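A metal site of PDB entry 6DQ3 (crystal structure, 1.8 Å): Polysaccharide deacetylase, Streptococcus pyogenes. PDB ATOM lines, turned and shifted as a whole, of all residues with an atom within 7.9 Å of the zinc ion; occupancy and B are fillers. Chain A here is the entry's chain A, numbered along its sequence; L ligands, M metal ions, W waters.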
ATOM      1  N   HIS A  15      -4.331  36.181  12.656  1.00  0.00           N
ATOM      2  CA  HIS A  15      -4.237  35.341  11.475  1.00  0.00           C
ATOM      3  C   HIS A  15      -4.662  36.186  10.287  1.00  0.00           C
ATOM      4  O   HIS A  15      -3.865  36.991   9.783  1.00  0.00           O
ATOM      5  CB  HIS A  15      -5.080  34.071  11.632  1.00  0.00           C
ATOM      6  CG  HIS A  15      -4.363  32.996  12.405  1.00  0.00           C
ATOM      7  ND1 HIS A  15      -4.254  33.016  13.775  1.00  0.00           N
ATOM      8  CD2 HIS A  15      -3.723  31.881  11.981  1.00  0.00           C
ATOM      9  CE1 HIS A  15      -3.579  31.952  14.176  1.00  0.00           C
ATOM     10  NE2 HIS A  15      -3.254  31.242  13.109  1.00  0.00           N
ATOM     11  N   PHE A  76       1.784  36.985  13.785  1.00  0.00           N
ATOM     12  CA  PHE A  76       0.866  36.552  12.736  1.00  0.00           C
ATOM     13  C   PHE A  76       1.341  35.187  12.242  1.00  0.00           C
ATOM     14  O   PHE A  76       2.512  35.035  11.872  1.00  0.00           O
ATOM     15  CB  PHE A  76       0.865  37.525  11.551  1.00  0.00           C
ATOM     16  CG  PHE A  76       0.227  38.851  11.839  1.00  0.00           C
ATOM     17  CD1 PHE A  76       0.831  39.766  12.693  1.00  0.00           C
ATOM     18  CD2 PHE A  76      -0.969  39.213  11.229  1.00  0.00           C
ATOM     19  CE1 PHE A  76       0.252  40.989  12.953  1.00  0.00           C
ATOM     20  CE2 PHE A  76      -1.552  40.442  11.482  1.00  0.00           C
ATOM     21  CZ  PHE A  76      -0.941  41.323  12.345  1.00  0.00           C
ATOM     22  N   ASP A  77       0.444  34.210  12.195  1.00  0.00           N
ATOM     23  CA  ASP A  77       0.814  32.893  11.706  1.00  0.00           C
ATOM     24  C   ASP A  77       0.415  32.701  10.238  1.00  0.00           C
ATOM     25  O   ASP A  77      -0.460  33.386   9.713  1.00  0.00           O
ATOM     26  CB  ASP A  77       0.152  31.785  12.550  1.00  0.00           C
ATOM     27  CG  ASP A  77       0.510  31.865  14.015  1.00  0.00           C
ATOM     28  OD1 ASP A  77       1.563  32.452  14.353  1.00  0.00           O
ATOM     29  OD2 ASP A  77      -0.251  31.338  14.847  1.00  0.00           O
ATOM     30  N   ASP A  78       1.125  31.769   9.594  1.00  0.00           N
ATOM     31  CA  ASP A  78       0.758  31.146   8.320  1.00  0.00           C
ATOM     32  C   ASP A  78       1.189  31.938   7.084  1.00  0.00           C
ATOM     33  O   ASP A  78       0.879  31.552   5.951  1.00  0.00           O
ATOM     34  CB  ASP A  78      -0.757  30.898   8.276  1.00  0.00           C
ATOM     35  CG  ASP A  78      -1.214  29.835   9.259  1.00  0.00           C
ATOM     36  OD1 ASP A  78      -0.342  29.152   9.818  1.00  0.00           O
ATOM     37  OD2 ASP A  78      -2.440  29.701   9.486  1.00  0.00           O
ATOM     38  N   SER A  79       1.937  33.013   7.302  1.00  0.00           N
ATOM     39  CA  SER A  79       2.568  33.795   6.232  1.00  0.00           C
ATOM     40  C   SER A  79       1.635  33.968   5.037  1.00  0.00           C
ATOM     41  O   SER A  79       1.972  33.668   3.892  1.00  0.00           O
ATOM     42  CB  SER A  79       3.891  33.148   5.815  1.00  0.00           C
ATOM     43  OG  SER A  79       3.767  31.742   5.661  1.00  0.00           O
ATOM     44  N   ASN A 101       5.060  34.177  11.373  1.00  0.00           N
ATOM     45  CA  ASN A 101       5.581  32.818  11.459  1.00  0.00           C
ATOM     46  C   ASN A 101       5.306  32.095  10.153  1.00  0.00           C
ATOM     47  O   ASN A 101       4.148  31.846   9.807  1.00  0.00           O
ATOM     48  CB  ASN A 101       4.968  32.134  12.670  1.00  0.00           C
ATOM     49  CG  ASN A 101       5.260  32.907  13.950  1.00  0.00           C
ATOM     50  OD1 ASN A 101       6.413  33.241  14.215  1.00  0.00           O
ATOM     51  ND2 ASN A 101       4.229  33.224  14.719  1.00  0.00           N
ATOM     52  N   ILE A 103       5.385  29.503   6.916  1.00  0.00           N
ATOM     53  CA  ILE A 103       5.322  28.147   6.393  1.00  0.00           C
ATOM     54  C   ILE A 103       6.235  28.119   5.170  1.00  0.00           C
ATOM     55  O   ILE A 103       5.835  28.539   4.081  1.00  0.00           O
ATOM     56  CB  ILE A 103       3.889  27.734   6.037  1.00  0.00           C
ATOM     57  CG1 ILE A 103       2.964  27.937   7.236  1.00  0.00           C
ATOM     58  CG2 ILE A 103       3.848  26.297   5.544  1.00  0.00           C
ATOM     59  CD1 ILE A 103       1.488  27.787   6.910  1.00  0.00           C
ATOM     60  N   HIS A 133       7.453  28.503  11.088  1.00  0.00           N
ATOM     61  CA  HIS A 133       6.165  27.834  11.215  1.00  0.00           C
ATOM     62  C   HIS A 133       6.181  26.505  10.472  1.00  0.00           C
ATOM     63  O   HIS A 133       5.158  26.084   9.923  1.00  0.00           O
ATOM     64  CB  HIS A 133       5.044  28.748  10.728  1.00  0.00           C
ATOM     65  CG  HIS A 133       3.704  28.443  11.321  1.00  0.00           C
ATOM     66  ND1 HIS A 133       3.541  27.989  12.613  1.00  0.00           N
ATOM     67  CD2 HIS A 133       2.459  28.565  10.802  1.00  0.00           C
ATOM     68  CE1 HIS A 133       2.250  27.821  12.865  1.00  0.00           C
ATOM     69  NE2 HIS A 133       1.565  28.163  11.776  1.00  0.00           N
ATOM     70  N   THR A 134       7.349  25.838  10.465  1.00  0.00           N
ATOM     71  CA  THR A 134       7.610  24.549   9.830  1.00  0.00           C
ATOM     72  C   THR A 134       7.626  24.644   8.308  1.00  0.00           C
ATOM     73  O   THR A 134       7.290  25.686   7.732  1.00  0.00           O
ATOM     74  CB  THR A 134       6.601  23.466  10.238  1.00  0.00           C
ATOM     75  OG1 THR A 134       5.384  23.625   9.511  1.00  0.00           O
ATOM     76  CG2 THR A 134       6.327  23.486  11.745  1.00  0.00           C
ATOM     77  N   HIS A 137       3.704  22.490   7.636  1.00  0.00           N
ATOM     78  CA  HIS A 137       2.617  22.729   8.579  1.00  0.00           C
ATOM     79  C   HIS A 137       1.934  21.424   9.010  1.00  0.00           C
ATOM     80  O   HIS A 137       0.693  21.359   9.039  1.00  0.00           O
ATOM     81  CB  HIS A 137       1.590  23.678   7.959  1.00  0.00           C
ATOM     82  CG  HIS A 137       0.778  24.461   8.951  1.00  0.00           C
ATOM     83  ND1 HIS A 137      -0.450  24.037   9.406  1.00  0.00           N
ATOM     84  CD2 HIS A 137       1.017  25.655   9.543  1.00  0.00           C
ATOM     85  CE1 HIS A 137      -0.936  24.935  10.254  1.00  0.00           C
ATOM     86  NE2 HIS A 137      -0.066  25.920  10.356  1.00  0.00           N
ATOM     87  N   PRO A 138       2.700  20.395   9.372  1.00  0.00           N
ATOM     88  CA  PRO A 138       2.078  19.201   9.958  1.00  0.00           C
ATOM     89  C   PRO A 138       1.679  19.432  11.410  1.00  0.00           C
ATOM     90  O   PRO A 138       2.108  20.386  12.064  1.00  0.00           O
ATOM     91  CB  PRO A 138       3.192  18.158   9.860  1.00  0.00           C
ATOM     92  CG  PRO A 138       4.441  18.976  10.080  1.00  0.00           C
ATOM     93  CD  PRO A 138       4.166  20.283   9.335  1.00  0.00           C
ATOM     94  N   ALA A 171       6.433  28.981  15.928  1.00  0.00           N
ATOM     95  CA  ALA A 171       5.035  28.784  16.311  1.00  0.00           C
ATOM     96  C   ALA A 171       4.636  27.378  15.863  1.00  0.00           C
ATOM     97  O   ALA A 171       4.770  27.047  14.682  1.00  0.00           O
ATOM     98  CB  ALA A 171       4.127  29.835  15.666  1.00  0.00           C
ATOM     99  N   TYR A 172       4.161  26.559  16.800  1.00  0.00           N
ATOM    100  CA  TYR A 172       3.795  25.186  16.452  1.00  0.00           C
ATOM    101  C   TYR A 172       2.476  25.175  15.691  1.00  0.00           C
ATOM    102  O   TYR A 172       1.526  25.838  16.114  1.00  0.00           O
ATOM    103  CB  TYR A 172       3.690  24.329  17.723  1.00  0.00           C
ATOM    104  CG  TYR A 172       4.916  24.473  18.577  1.00  0.00           C
ATOM    105  CD1 TYR A 172       6.156  24.064  18.119  1.00  0.00           C
ATOM    106  CD2 TYR A 172       4.848  25.058  19.835  1.00  0.00           C
ATOM    107  CE1 TYR A 172       7.282  24.220  18.881  1.00  0.00           C
ATOM    108  CE2 TYR A 172       5.968  25.221  20.607  1.00  0.00           C
ATOM    109  CZ  TYR A 172       7.191  24.801  20.120  1.00  0.00           C
ATOM    110  OH  TYR A 172       8.317  24.957  20.882  1.00  0.00           O
ATOM    111  N   PRO A 173       2.381  24.456  14.577  1.00  0.00           N
ATOM    112  CA  PRO A 173       1.125  24.430  13.823  1.00  0.00           C
ATOM    113  C   PRO A 173      -0.034  23.966  14.694  1.00  0.00           C
ATOM    114  O   PRO A 173       0.024  22.916  15.348  1.00  0.00           O
ATOM    115  CB  PRO A 173       1.406  23.461  12.675  1.00  0.00           C
ATOM    116  CG  PRO A 173       2.881  23.627  12.441  1.00  0.00           C
ATOM    117  CD  PRO A 173       3.479  23.805  13.831  1.00  0.00           C
ATOM    118  N   SER A 174      -1.096  24.764  14.696  1.00  0.00           N
ATOM    119  CA  SER A 174      -2.313  24.507  15.466  1.00  0.00           C
ATOM    120  C   SER A 174      -2.057  24.437  16.960  1.00  0.00           C
ATOM    121  O   SER A 174      -2.908  23.967  17.722  1.00  0.00           O
ATOM    122  CB  SER A 174      -2.993  23.226  14.966  1.00  0.00           C
ATOM    123  OG  SER A 174      -3.368  23.366  13.612  1.00  0.00           O
ATOM    124  N   GLY A 175      -0.902  24.935  17.407  1.00  0.00           N
ATOM    125  CA  GLY A 175      -0.574  24.930  18.811  1.00  0.00           C
ATOM    126  C   GLY A 175      -0.287  23.570  19.391  1.00  0.00           C
ATOM    127  O   GLY A 175      -0.288  23.426  20.615  1.00  0.00           O
ATOM    128  N   THR A 196      -0.945  28.065  21.217  1.00  0.00           N
ATOM    129  CA  THR A 196      -2.259  28.693  21.188  1.00  0.00           C
ATOM    130  C   THR A 196      -2.951  28.661  22.547  1.00  0.00           C
ATOM    131  O   THR A 196      -4.167  28.894  22.629  1.00  0.00           O
ATOM    132  CB  THR A 196      -3.157  28.053  20.113  1.00  0.00           C
ATOM    133  OG1 THR A 196      -3.332  26.651  20.373  1.00  0.00           O
ATOM    134  CG2 THR A 196      -2.540  28.239  18.720  1.00  0.00           C
ATOM    135  N   ARG A 212      -0.312  32.788  24.176  1.00  0.00           N
ATOM    136  CA  ARG A 212      -0.665  33.898  23.297  1.00  0.00           C
ATOM    137  C   ARG A 212      -2.115  34.312  23.530  1.00  0.00           C
ATOM    138  O   ARG A 212      -2.915  33.545  24.072  1.00  0.00           O
ATOM    139  CB  ARG A 212      -0.447  33.532  21.819  1.00  0.00           C
ATOM    140  CG  ARG A 212       1.013  33.380  21.447  1.00  0.00           C
ATOM    141  CD  ARG A 212       1.236  33.490  19.945  1.00  0.00           C
ATOM    142  NE  ARG A 212       0.873  32.269  19.239  1.00  0.00           N
ATOM    143  CZ  ARG A 212       0.918  32.118  17.921  1.00  0.00           C
ATOM    144  NH1 ARG A 212       1.316  33.127  17.151  1.00  0.00           N
ATOM    145  NH2 ARG A 212       0.572  30.959  17.370  1.00  0.00           N
HETATM  146  C1  LIG L   1      -1.342  28.093  13.701  1.00  0.00           C
HETATM  147  O1  LIG L   1      -1.567  29.078  12.971  1.00  0.00           O
HETATM  148  O2  LIG L   1      -1.049  26.947  13.316  1.00  0.00           O
HETATM  149  C2  LIG L   1      -1.421  28.320  15.126  1.00  0.00           C
HETATM  150 ZN    ZN M   1      -0.507  27.713  11.290  1.00  0.00          ZN
HETATM  151  O   HOH W   1      -2.816  27.444  10.793  1.00  0.00           O
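The backbone carbonyl oxygen (O) of Ala 171 is in hydrogen-bond range of a ring nitrogen (ND1) of His 133.
The backbone carbonyl oxygen (O) of Asn 101 lies within hydrogen-bond range of the backbone NH (N) of Asp 78, at 3.0 Å.
The backbone NH (N) of His 137 lies within hydrogen-bond range of the side-chain hydroxyl (OG1) of Thr 134, at 2.8 Å.
Of the 18 residues printed, 3 come within 4 Å of the zinc ion.
The nearest printed residue that does not touch the zinc ion is Asp 77 (4.3 Å).
The zinc ion is bound by the side-chain carboxylate of Asp 78, a ring nitrogen (NE2) of His 137, a ring nitrogen (NE2) of His 133, an oxygen (O2) of the ligand, water W1 and an oxygen (O1) of the ligand.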
